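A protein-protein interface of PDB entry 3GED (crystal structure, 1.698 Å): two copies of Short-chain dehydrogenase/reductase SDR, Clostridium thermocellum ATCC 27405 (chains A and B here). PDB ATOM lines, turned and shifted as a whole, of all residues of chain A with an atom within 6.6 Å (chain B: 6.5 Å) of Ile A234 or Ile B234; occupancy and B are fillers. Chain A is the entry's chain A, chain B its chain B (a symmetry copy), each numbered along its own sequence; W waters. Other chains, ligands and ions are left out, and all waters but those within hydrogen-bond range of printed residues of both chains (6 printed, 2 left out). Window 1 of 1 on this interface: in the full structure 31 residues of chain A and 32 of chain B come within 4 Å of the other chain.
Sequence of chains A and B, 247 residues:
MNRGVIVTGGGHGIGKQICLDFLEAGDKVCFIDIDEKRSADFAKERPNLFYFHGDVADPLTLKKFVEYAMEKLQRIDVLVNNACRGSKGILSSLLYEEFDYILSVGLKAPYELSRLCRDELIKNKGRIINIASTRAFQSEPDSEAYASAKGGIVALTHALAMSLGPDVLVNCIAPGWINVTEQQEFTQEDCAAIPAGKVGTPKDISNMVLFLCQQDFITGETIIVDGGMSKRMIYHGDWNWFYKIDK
Water W5 bridges OD2 of Asp B238 (2.4 Å) and OE2 of Glu A140 (2.8 Å).
Water W6 bridges the side-chain carboxylate of Asp A238 and the side-chain carboxylate of Glu B140.
Water W3 lies within hydrogen-bond range of O of Arg B232, O of Met B229, NE2 of Gln B138 and NE2 of Gln A138.
Water W2 lies within hydrogen-bond range of O of Arg A232 (2.9 Å), O of Met A229 (2.9 Å), NE2 of Gln A138 (3.2 Å) and NE2 of Gln B138 (3.3 Å).
Water W4 lies within hydrogen-bond range of the backbone NH of His B236 (3.0 Å) and the side-chain sulfur of Met A229 (3.4 Å).
Water W1 lies within hydrogen-bond range of N of His A236 (3.0 Å) and SD of Met B229 (3.4 Å).
Gln A138 touches its own counterpart, Gln B138.
Ser A139 touches Met B233, and with the chains exchanged Met A233 touches Ser B139.
Ile B234 touches its own counterpart, Ile A234.
Phe B242 touches its own counterpart, Phe A242.
13 positions are printed for both chains.
Of the 27 pairs that touch across the chains among the printed residues, 27 have their exchanged pair printed and touching as well.
The side-chain amide nitrogen (NE2) of Gln B138 lies close to the side-chain amide nitrogen (NE2) of Gln A138, at 3.3 Å.
The backbone carbonyl oxygen of Ser A139 is in hydrogen-bond range of the backbone NH of Met B233 (2.8 Å).
The backbone NH (N) of Met A233 sits at hydrogen-bond distance from the backbone carbonyl oxygen (O) of Ser B139, at 2.8 Å.
The backbone NH (N) of Phe A242 sits at hydrogen-bond distance from the backbone carbonyl oxygen (O) of Phe B242 (2.8 Å).
Hydrophobic or aromatic side chains of chain A within 4 Å of the printed part of chain B: Ala A193, Met A229, Met A233, Ile A234, Tyr A235, His A236, Trp A241 and Phe A242.
Printed residues of chain B that touch a printed residue of chain A: Gln B138, Ser B139, Glu B140, Ala B193, Met B229, Arg B232, Met B233, Ile B234, Tyr B235, His B236, Asp B238, Trp B241 and Phe B242.
Hydrophobic or aromatic side chains of chain B that line the printed part of chain A: Ala B193, Met B229, Met B233, Ile B234, Tyr B235, His B236 and Trp B241.
Of chain B, only Met B229, Ile B234 and Trp B241 come within 4 Å of Ile A234.
Of the printed residues of chain A, Glu B140 touches Met A233 (3.2 Å) and Asp A238 (3.6 Å).
Ile B234 touches three residues of chain A.
Of the printed residues of chain A, His B236 touches Ala A193 and Trp A241.
Printed residues of chain A within 4 Å of Asp B238: Glu A140 (3.6 Å).
The nearest residue of chain B that does not touch Ile A234 is Glu B140 (5.0 Å).
The nearest printed residue of chain A that does not touch Asp B238 is Trp A241 (6.9 Å).
Among the printed residues, pairs that only touch across the chains: Gln A138 with Arg B232 (3.6 Å), Gln A138 with Met B233 (3.6 Å), Ser A139 with Arg B232 (3.5 Å), Glu A140 with Met B233 (3.3 Å), Glu A140 with Asp B238 (3.6 Å), Ala A193 with His B236 (3.7 Å), Met A229 with Ile B234 (3.6 Å), Met A229 with Tyr B235 (3.7 Å), Arg A232 with Gln B138 (3.6 Å), Arg A232 with Ser B139 (3.5 Å), Met A233 with Gln B138 (3.7 Å), Met A233 with Glu B140 (3.2 Å), Ile A234 with Met B229 (3.6 Å), Ile A234 with Ile B234 (3.8 Å), Ile A234 with Trp B241 (3.5 Å), Tyr A235 with Met B229 (3.7 Å), His A236 with Ala B193 (3.7 Å), His A236 with Trp B241 (3.6 Å), Asp A238 with Glu B140 (3.6 Å), Trp A241 with Ile B234 (3.6 Å), Trp A241 with His B236 (3.5 Å), Trp A241 with Phe B242 (3.6 Å) and Phe A242 with Trp B241 (3.5 Å).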
ATOM      1  N   GLN A 138      -8.594 -15.461  14.824  1.00  0.00           N
ATOM      2  CA  GLN A 138      -9.676 -15.219  13.850  1.00  0.00           C
ATOM      3  C   GLN A 138      -9.070 -15.200  12.464  1.00  0.00           C
ATOM      4  O   GLN A 138      -7.877 -14.929  12.312  1.00  0.00           O
ATOM      5  CB  GLN A 138     -10.283 -13.848  14.078  1.00  0.00           C
ATOM      6  CG  GLN A 138     -11.097 -13.736  15.351  1.00  0.00           C
ATOM      7  CD  GLN A 138     -11.491 -12.266  15.523  1.00  0.00           C
ATOM      8  OE1 GLN A 138     -10.616 -11.417  15.586  1.00  0.00           O
ATOM      9  NE2 GLN A 138     -12.791 -11.965  15.501  1.00  0.00           N
ATOM     10  N   SER A 139      -9.867 -15.481  11.445  1.00  0.00           N
ATOM     11  CA  SER A 139      -9.308 -15.543  10.075  1.00  0.00           C
ATOM     12  C   SER A 139     -10.089 -14.740   9.067  1.00  0.00           C
ATOM     13  O   SER A 139     -11.297 -14.637   9.156  1.00  0.00           O
ATOM     14  CB  SER A 139      -9.255 -16.997   9.560  1.00  0.00           C
ATOM     15  OG  SER A 139      -8.266 -17.733  10.250  1.00  0.00           O
ATOM     16  N   GLU A 140      -9.369 -14.196   8.083  1.00  0.00           N
ATOM     17  CA  GLU A 140     -10.006 -13.832   6.806  1.00  0.00           C
ATOM     18  C   GLU A 140      -9.808 -15.021   5.868  1.00  0.00           C
ATOM     19  O   GLU A 140      -8.956 -15.871   6.114  1.00  0.00           O
ATOM     20  CB  GLU A 140      -9.306 -12.603   6.222  1.00  0.00           C
ATOM     21  CG  GLU A 140      -9.591 -11.341   7.027  1.00  0.00           C
ATOM     22  CD  GLU A 140      -8.928 -10.099   6.472  1.00  0.00           C
ATOM     23  OE1 GLU A 140      -7.740 -10.175   6.063  1.00  0.00           O
ATOM     24  OE2 GLU A 140      -9.600  -9.040   6.472  1.00  0.00           O
ATOM     25  N   ALA A 193     -12.910   2.518  12.265  1.00  0.00           N
ATOM     26  CA  ALA A 193     -13.377   1.127  12.375  1.00  0.00           C
ATOM     27  C   ALA A 193     -12.671   0.377  13.508  1.00  0.00           C
ATOM     28  O   ALA A 193     -13.224  -0.569  14.091  1.00  0.00           O
ATOM     29  CB  ALA A 193     -13.202   0.404  11.018  1.00  0.00           C
ATOM     30  N   MET A 229      -9.707  -4.578  17.985  1.00  0.00           N
ATOM     31  CA  MET A 229     -10.456  -5.083  16.841  1.00  0.00           C
ATOM     32  C   MET A 229     -11.051  -6.469  17.056  1.00  0.00           C
ATOM     33  O   MET A 229     -12.195  -6.714  16.668  1.00  0.00           O
ATOM     34  CB  MET A 229      -9.569  -5.067  15.581  1.00  0.00           C
ATOM     35  CG  MET A 229     -10.376  -5.154  14.265  1.00  0.00           C
ATOM     36  SD  MET A 229     -11.338  -3.635  13.996  1.00  0.00           S
ATOM     37  CE  MET A 229     -12.994  -4.293  13.933  1.00  0.00           C
ATOM     38  N   ARG A 232     -14.346  -6.640  18.936  1.00  0.00           N
ATOM     39  CA  ARG A 232     -15.534  -6.012  18.402  1.00  0.00           C
ATOM     40  C   ARG A 232     -16.438  -7.047  17.738  1.00  0.00           C
ATOM     41  O   ARG A 232     -16.077  -7.656  16.706  1.00  0.00           O
ATOM     42  CB  ARG A 232     -15.136  -4.884  17.419  1.00  0.00           C
ATOM     43  CG  ARG A 232     -16.360  -4.172  16.772  1.00  0.00           C
ATOM     44  CD  ARG A 232     -17.263  -3.488  17.820  1.00  0.00           C
ATOM     45  NE  ARG A 232     -17.864  -2.267  17.256  1.00  0.00           N
ATOM     46  CZ  ARG A 232     -18.890  -2.236  16.409  1.00  0.00           C
ATOM     47  NH1 ARG A 232     -19.301  -1.063  15.933  1.00  0.00           N
ATOM     48  NH2 ARG A 232     -19.524  -3.362  16.048  1.00  0.00           N
ATOM     49  N   MET A 233     -17.637  -7.226  18.297  1.00  0.00           N
ATOM     50  CA  MET A 233     -18.621  -8.079  17.630  1.00  0.00           C
ATOM     51  C   MET A 233     -19.234  -7.329  16.462  1.00  0.00           C
ATOM     52  O   MET A 233     -19.667  -6.198  16.622  1.00  0.00           O
ATOM     53  CB  MET A 233     -19.721  -8.463  18.611  1.00  0.00           C
ATOM     54  CG  MET A 233     -20.881  -9.180  17.917  1.00  0.00           C
ATOM     55  SD  MET A 233     -22.038  -9.958  19.073  1.00  0.00           S
ATOM     56  CE  MET A 233     -20.984 -11.267  19.755  1.00  0.00           C
ATOM     57  N   ILE A 234     -19.256  -7.964  15.292  1.00  0.00           N
ATOM     58  CA  ILE A 234     -19.689  -7.338  14.063  1.00  0.00           C
ATOM     59  C   ILE A 234     -20.730  -8.209  13.368  1.00  0.00           C
ATOM     60  O   ILE A 234     -20.473  -9.371  13.034  1.00  0.00           O
ATOM     61  CB  ILE A 234     -18.501  -7.086  13.140  1.00  0.00           C
ATOM     62  CG1 ILE A 234     -17.577  -6.048  13.795  1.00  0.00           C
ATOM     63  CG2 ILE A 234     -18.989  -6.681  11.722  1.00  0.00           C
ATOM     64  CD1 ILE A 234     -16.163  -5.958  13.161  1.00  0.00           C
ATOM     65  N   TYR A 235     -21.916  -7.633  13.183  1.00  0.00           N
ATOM     66  CA  TYR A 235     -22.969  -8.238  12.374  1.00  0.00           C
ATOM     67  C   TYR A 235     -23.417  -7.261  11.316  1.00  0.00           C
ATOM     68  O   TYR A 235     -23.524  -6.069  11.573  1.00  0.00           O
ATOM     69  CB  TYR A 235     -24.182  -8.631  13.233  1.00  0.00           C
ATOM     70  CG  TYR A 235     -24.009  -9.979  13.907  1.00  0.00           C
ATOM     71  CD1 TYR A 235     -23.303 -10.085  15.115  1.00  0.00           C
ATOM     72  CD2 TYR A 235     -24.479 -11.148  13.312  1.00  0.00           C
ATOM     73  CE1 TYR A 235     -23.088 -11.338  15.735  1.00  0.00           C
ATOM     74  CE2 TYR A 235     -24.264 -12.410  13.922  1.00  0.00           C
ATOM     75  CZ  TYR A 235     -23.585 -12.484  15.137  1.00  0.00           C
ATOM     76  OH  TYR A 235     -23.354 -13.700  15.781  1.00  0.00           O
ATOM     77  N   HIS A 236     -23.662  -7.773  10.115  1.00  0.00           N
ATOM     78  CA  HIS A 236     -24.051  -6.943   9.000  1.00  0.00           C
ATOM     79  C   HIS A 236     -25.271  -6.078   9.341  1.00  0.00           C
ATOM     80  O   HIS A 236     -26.283  -6.587   9.837  1.00  0.00           O
ATOM     81  CB  HIS A 236     -24.398  -7.823   7.814  1.00  0.00           C
ATOM     82  CG  HIS A 236     -25.162  -7.094   6.765  1.00  0.00           C
ATOM     83  ND1 HIS A 236     -24.562  -6.203   5.908  1.00  0.00           N
ATOM     84  CD2 HIS A 236     -26.483  -7.083   6.467  1.00  0.00           C
ATOM     85  CE1 HIS A 236     -25.481  -5.691   5.102  1.00  0.00           C
ATOM     86  NE2 HIS A 236     -26.656  -6.201   5.434  1.00  0.00           N
ATOM     87  N   ASP A 238     -25.557  -3.636  11.554  1.00  0.00           N
ATOM     88  CA  ASP A 238     -25.679  -3.195  12.930  1.00  0.00           C
ATOM     89  C   ASP A 238     -24.434  -2.423  13.338  1.00  0.00           C
ATOM     90  O   ASP A 238     -23.309  -2.769  12.936  1.00  0.00           O
ATOM     91  CB  ASP A 238     -25.861  -4.402  13.849  1.00  0.00           C
ATOM     92  CG  ASP A 238     -27.086  -5.233  13.487  1.00  0.00           C
ATOM     93  OD1 ASP A 238     -28.066  -4.643  13.005  1.00  0.00           O
ATOM     94  OD2 ASP A 238     -27.084  -6.468  13.693  1.00  0.00           O
ATOM     95  N   TRP A 241     -21.516  -1.334  10.644  1.00  0.00           N
ATOM     96  CA  TRP A 241     -20.822  -2.289   9.786  1.00  0.00           C
ATOM     97  C   TRP A 241     -21.729  -2.913   8.734  1.00  0.00           C
ATOM     98  O   TRP A 241     -22.886  -3.218   9.006  1.00  0.00           O
ATOM     99  CB  TRP A 241     -20.212  -3.417  10.639  1.00  0.00           C
ATOM    100  CG  TRP A 241     -18.913  -3.031  11.306  1.00  0.00           C
ATOM    101  CD1 TRP A 241     -18.742  -2.592  12.586  1.00  0.00           C
ATOM    102  CD2 TRP A 241     -17.615  -3.088  10.720  1.00  0.00           C
ATOM    103  NE1 TRP A 241     -17.403  -2.365  12.834  1.00  0.00           N
ATOM    104  CE2 TRP A 241     -16.691  -2.654  11.700  1.00  0.00           C
ATOM    105  CE3 TRP A 241     -17.144  -3.451   9.450  1.00  0.00           C
ATOM    106  CZ2 TRP A 241     -15.329  -2.580  11.462  1.00  0.00           C
ATOM    107  CZ3 TRP A 241     -15.784  -3.363   9.204  1.00  0.00           C
ATOM    108  CH2 TRP A 241     -14.886  -2.937  10.217  1.00  0.00           C
ATOM    109  N   PHE A 242     -21.191  -3.137   7.538  1.00  0.00           N
ATOM    110  CA  PHE A 242     -21.995  -3.642   6.438  1.00  0.00           C
ATOM    111  C   PHE A 242     -21.198  -4.610   5.586  1.00  0.00           C
ATOM    112  O   PHE A 242     -20.002  -4.399   5.341  1.00  0.00           O
ATOM    113  CB  PHE A 242     -22.513  -2.476   5.558  1.00  0.00           C
ATOM    114  CG  PHE A 242     -23.357  -1.491   6.315  1.00  0.00           C
ATOM    115  CD1 PHE A 242     -24.742  -1.618   6.341  1.00  0.00           C
ATOM    116  CD2 PHE A 242     -22.766  -0.471   7.058  1.00  0.00           C
ATOM    117  CE1 PHE A 242     -25.526  -0.733   7.071  1.00  0.00           C
ATOM    118  CE2 PHE A 242     -23.544   0.423   7.792  1.00  0.00           C
ATOM    119  CZ  PHE A 242     -24.925   0.291   7.795  1.00  0.00           C
ATOM    120  N   GLN B 138     -17.160 -11.226  22.704  1.00  0.00           N
ATOM    121  CA  GLN B 138     -16.963  -9.997  21.908  1.00  0.00           C
ATOM    122  C   GLN B 138     -18.154  -9.103  22.137  1.00  0.00           C
ATOM    123  O   GLN B 138     -19.215  -9.593  22.483  1.00  0.00           O
ATOM    124  CB  GLN B 138     -16.970 -10.323  20.438  1.00  0.00           C
ATOM    125  CG  GLN B 138     -15.783 -11.136  19.928  1.00  0.00           C
ATOM    126  CD  GLN B 138     -16.037 -11.565  18.490  1.00  0.00           C
ATOM    127  OE1 GLN B 138     -17.000 -12.297  18.236  1.00  0.00           O
ATOM    128  NE2 GLN B 138     -15.223 -11.079  17.529  1.00  0.00           N
ATOM    129  N   SER B 139     -18.003  -7.804  21.890  1.00  0.00           N
ATOM    130  CA  SER B 139     -19.094  -6.867  22.201  1.00  0.00           C
ATOM    131  C   SER B 139     -19.400  -5.924  21.067  1.00  0.00           C
ATOM    132  O   SER B 139     -18.511  -5.497  20.344  1.00  0.00           O
ATOM    133  CB  SER B 139     -18.750  -6.019  23.446  1.00  0.00           C
ATOM    134  OG  SER B 139     -18.867  -6.767  24.646  1.00  0.00           O
ATOM    135  N   GLU B 140     -20.680  -5.590  20.943  1.00  0.00           N
ATOM    136  CA  GLU B 140     -21.089  -4.363  20.257  1.00  0.00           C
ATOM    137  C   GLU B 140     -21.227  -3.281  21.338  1.00  0.00           C
ATOM    138  O   GLU B 140     -21.317  -3.583  22.509  1.00  0.00           O
ATOM    139  CB  GLU B 140     -22.430  -4.581  19.561  1.00  0.00           C
ATOM    140  CG  GLU B 140     -22.327  -5.490  18.333  1.00  0.00           C
ATOM    141  CD  GLU B 140     -23.667  -5.701  17.652  1.00  0.00           C
ATOM    142  OE1 GLU B 140     -24.657  -5.902  18.378  1.00  0.00           O
ATOM    143  OE2 GLU B 140     -23.722  -5.661  16.400  1.00  0.00           O
ATOM    144  N   ALA B 193     -23.250 -12.811   5.152  1.00  0.00           N
ATOM    145  CA  ALA B 193     -22.252 -12.266   6.100  1.00  0.00           C
ATOM    146  C   ALA B 193     -21.823 -13.276   7.142  1.00  0.00           C
ATOM    147  O   ALA B 193     -20.702 -13.189   7.682  1.00  0.00           O
ATOM    148  CB  ALA B 193     -22.766 -10.997   6.767  1.00  0.00           C
ATOM    149  N   MET B 229     -19.372 -16.833  13.026  1.00  0.00           N
ATOM    150  CA  MET B 229     -19.249 -15.373  13.006  1.00  0.00           C
ATOM    151  C   MET B 229     -18.079 -14.845  13.866  1.00  0.00           C
ATOM    152  O   MET B 229     -17.366 -13.947  13.440  1.00  0.00           O
ATOM    153  CB  MET B 229     -20.586 -14.723  13.435  1.00  0.00           C
ATOM    154  CG  MET B 229     -20.702 -13.228  13.007  1.00  0.00           C
ATOM    155  SD  MET B 229     -20.747 -12.989  11.219  1.00  0.00           S
ATOM    156  CE  MET B 229     -19.239 -12.064  10.926  1.00  0.00           C
ATOM    157  N   ARG B 232     -14.616 -14.955  12.294  1.00  0.00           N
ATOM    158  CA  ARG B 232     -14.292 -14.174  11.114  1.00  0.00           C
ATOM    159  C   ARG B 232     -13.548 -12.888  11.494  1.00  0.00           C
ATOM    160  O   ARG B 232     -14.117 -11.992  12.142  1.00  0.00           O
ATOM    161  CB  ARG B 232     -15.605 -13.861  10.341  1.00  0.00           C
ATOM    162  CG  ARG B 232     -15.394 -13.011   9.053  1.00  0.00           C
ATOM    163  CD  ARG B 232     -14.509 -13.720   8.049  1.00  0.00           C
ATOM    164  NE  ARG B 232     -14.909 -13.350   6.674  1.00  0.00           N
ATOM    165  CZ  ARG B 232     -14.626 -12.192   6.082  1.00  0.00           C
ATOM    166  NH1 ARG B 232     -15.052 -11.960   4.840  1.00  0.00           N
ATOM    167  NH2 ARG B 232     -13.851 -11.292   6.693  1.00  0.00           N
ATOM    168  N   MET B 233     -12.280 -12.779  11.072  1.00  0.00           N
ATOM    169  CA  MET B 233     -11.568 -11.514  11.182  1.00  0.00           C
ATOM    170  C   MET B 233     -12.118 -10.515  10.185  1.00  0.00           C
ATOM    171  O   MET B 233     -12.240 -10.823   8.996  1.00  0.00           O
ATOM    172  CB  MET B 233     -10.072 -11.722  10.922  1.00  0.00           C
ATOM    173  CG  MET B 233      -9.309 -10.398  10.966  1.00  0.00           C
ATOM    174  SD  MET B 233      -7.536 -10.698  10.986  1.00  0.00           S
ATOM    175  CE  MET B 233      -7.366 -11.348  12.674  1.00  0.00           C
ATOM    176  N   ILE B 234     -12.463  -9.326  10.665  1.00  0.00           N
ATOM    177  CA  ILE B 234     -13.056  -8.306   9.842  1.00  0.00           C
ATOM    178  C   ILE B 234     -12.317  -6.979  10.003  1.00  0.00           C
ATOM    179  O   ILE B 234     -12.206  -6.456  11.103  1.00  0.00           O
ATOM    180  CB  ILE B 234     -14.546  -8.108  10.205  1.00  0.00           C
ATOM    181  CG1 ILE B 234     -15.336  -9.392   9.914  1.00  0.00           C
ATOM    182  CG2 ILE B 234     -15.104  -6.860   9.506  1.00  0.00           C
ATOM    183  CD1 ILE B 234     -16.706  -9.431  10.568  1.00  0.00           C
ATOM    184  N   TYR B 235     -11.818  -6.459   8.890  1.00  0.00           N
ATOM    185  CA  TYR B 235     -11.233  -5.124   8.816  1.00  0.00           C
ATOM    186  C   TYR B 235     -11.899  -4.327   7.730  1.00  0.00           C
ATOM    187  O   TYR B 235     -12.196  -4.854   6.662  1.00  0.00           O
ATOM    188  CB  TYR B 235      -9.737  -5.208   8.517  1.00  0.00           C
ATOM    189  CG  TYR B 235      -8.918  -5.426   9.762  1.00  0.00           C
ATOM    190  CD1 TYR B 235      -8.702  -6.717  10.272  1.00  0.00           C
ATOM    191  CD2 TYR B 235      -8.404  -4.343  10.466  1.00  0.00           C
ATOM    192  CE1 TYR B 235      -7.962  -6.923  11.462  1.00  0.00           C
ATOM    193  CE2 TYR B 235      -7.640  -4.542  11.632  1.00  0.00           C
ATOM    194  CZ  TYR B 235      -7.442  -5.830  12.123  1.00  0.00           C
ATOM    195  OH  TYR B 235      -6.708  -6.059  13.277  1.00  0.00           O
ATOM    196  N   HIS B 236     -12.153  -3.048   8.000  1.00  0.00           N
ATOM    197  CA  HIS B 236     -12.809  -2.204   7.041  1.00  0.00           C
ATOM    198  C   HIS B 236     -12.139  -2.245   5.658  1.00  0.00           C
ATOM    199  O   HIS B 236     -10.917  -2.084   5.532  1.00  0.00           O
ATOM    200  CB  HIS B 236     -12.825  -0.767   7.540  1.00  0.00           C
ATOM    201  CG  HIS B 236     -13.125   0.213   6.464  1.00  0.00           C
ATOM    202  ND1 HIS B 236     -14.389   0.372   5.948  1.00  0.00           N
ATOM    203  CD2 HIS B 236     -12.316   1.048   5.770  1.00  0.00           C
ATOM    204  CE1 HIS B 236     -14.351   1.296   4.996  1.00  0.00           C
ATOM    205  NE2 HIS B 236     -13.103   1.708   4.865  1.00  0.00           N
ATOM    206  N   ASP B 238     -11.767  -4.666   3.561  1.00  0.00           N
ATOM    207  CA  ASP B 238     -11.183  -5.940   3.144  1.00  0.00           C
ATOM    208  C   ASP B 238     -12.218  -7.062   3.144  1.00  0.00           C
ATOM    209  O   ASP B 238     -13.102  -7.123   4.018  1.00  0.00           O
ATOM    210  CB  ASP B 238     -10.036  -6.340   4.074  1.00  0.00           C
ATOM    211  CG  ASP B 238      -8.937  -5.294   4.138  1.00  0.00           C
ATOM    212  OD1 ASP B 238      -8.711  -4.632   3.113  1.00  0.00           O
ATOM    213  OD2 ASP B 238      -8.299  -5.139   5.208  1.00  0.00           O
ATOM    214  N   TRP B 241     -16.241  -6.457   3.758  1.00  0.00           N
ATOM    215  CA  TRP B 241     -16.799  -5.724   4.886  1.00  0.00           C
ATOM    216  C   TRP B 241     -16.391  -4.263   4.857  1.00  0.00           C
ATOM    217  O   TRP B 241     -15.245  -3.920   4.507  1.00  0.00           O
ATOM    218  CB  TRP B 241     -16.280  -6.336   6.189  1.00  0.00           C
ATOM    219  CG  TRP B 241     -16.978  -7.581   6.559  1.00  0.00           C
ATOM    220  CD1 TRP B 241     -16.590  -8.872   6.301  1.00  0.00           C
ATOM    221  CD2 TRP B 241     -18.216  -7.667   7.261  1.00  0.00           C
ATOM    222  NE1 TRP B 241     -17.509  -9.747   6.817  1.00  0.00           N
ATOM    223  CE2 TRP B 241     -18.516  -9.038   7.408  1.00  0.00           C
ATOM    224  CE3 TRP B 241     -19.098  -6.713   7.782  1.00  0.00           C
ATOM    225  CZ2 TRP B 241     -19.659  -9.488   8.075  1.00  0.00           C
ATOM    226  CZ3 TRP B 241     -20.236  -7.157   8.440  1.00  0.00           C
ATOM    227  CH2 TRP B 241     -20.514  -8.532   8.563  1.00  0.00           C
ATOM    228  N   PHE B 242     -17.335  -3.416   5.232  1.00  0.00           N
ATOM    229  CA  PHE B 242     -17.123  -1.981   5.234  1.00  0.00           C
ATOM    230  C   PHE B 242     -17.759  -1.311   6.446  1.00  0.00           C
ATOM    231  O   PHE B 242     -18.864  -1.664   6.877  1.00  0.00           O
ATOM    232  CB  PHE B 242     -17.646  -1.340   3.936  1.00  0.00           C
ATOM    233  CG  PHE B 242     -17.092  -1.963   2.689  1.00  0.00           C
ATOM    234  CD1 PHE B 242     -16.026  -1.376   2.015  1.00  0.00           C
ATOM    235  CD2 PHE B 242     -17.629  -3.151   2.192  1.00  0.00           C
ATOM    236  CE1 PHE B 242     -15.504  -1.955   0.861  1.00  0.00           C
ATOM    237  CE2 PHE B 242     -17.112  -3.741   1.038  1.00  0.00           C
ATOM    238  CZ  PHE B 242     -16.055  -3.137   0.365  1.00  0.00           C
HETATM  239  O   HOH W   1     -22.992 -10.697  10.050  1.00  0.00           O
HETATM  240  O   HOH W   2     -13.772  -8.904  15.530  1.00  0.00           O
HETATM  241  O   HOH W   3     -15.846 -11.622  14.366  1.00  0.00           O
HETATM  242  O   HOH W   4     -11.336  -2.408  10.778  1.00  0.00           O
HETATM  243  O   HOH W   5      -7.497  -7.263   6.041  1.00  0.00           O
HETATM  244  O   HOH W   6     -26.298  -6.891  16.184  1.00  0.00           O
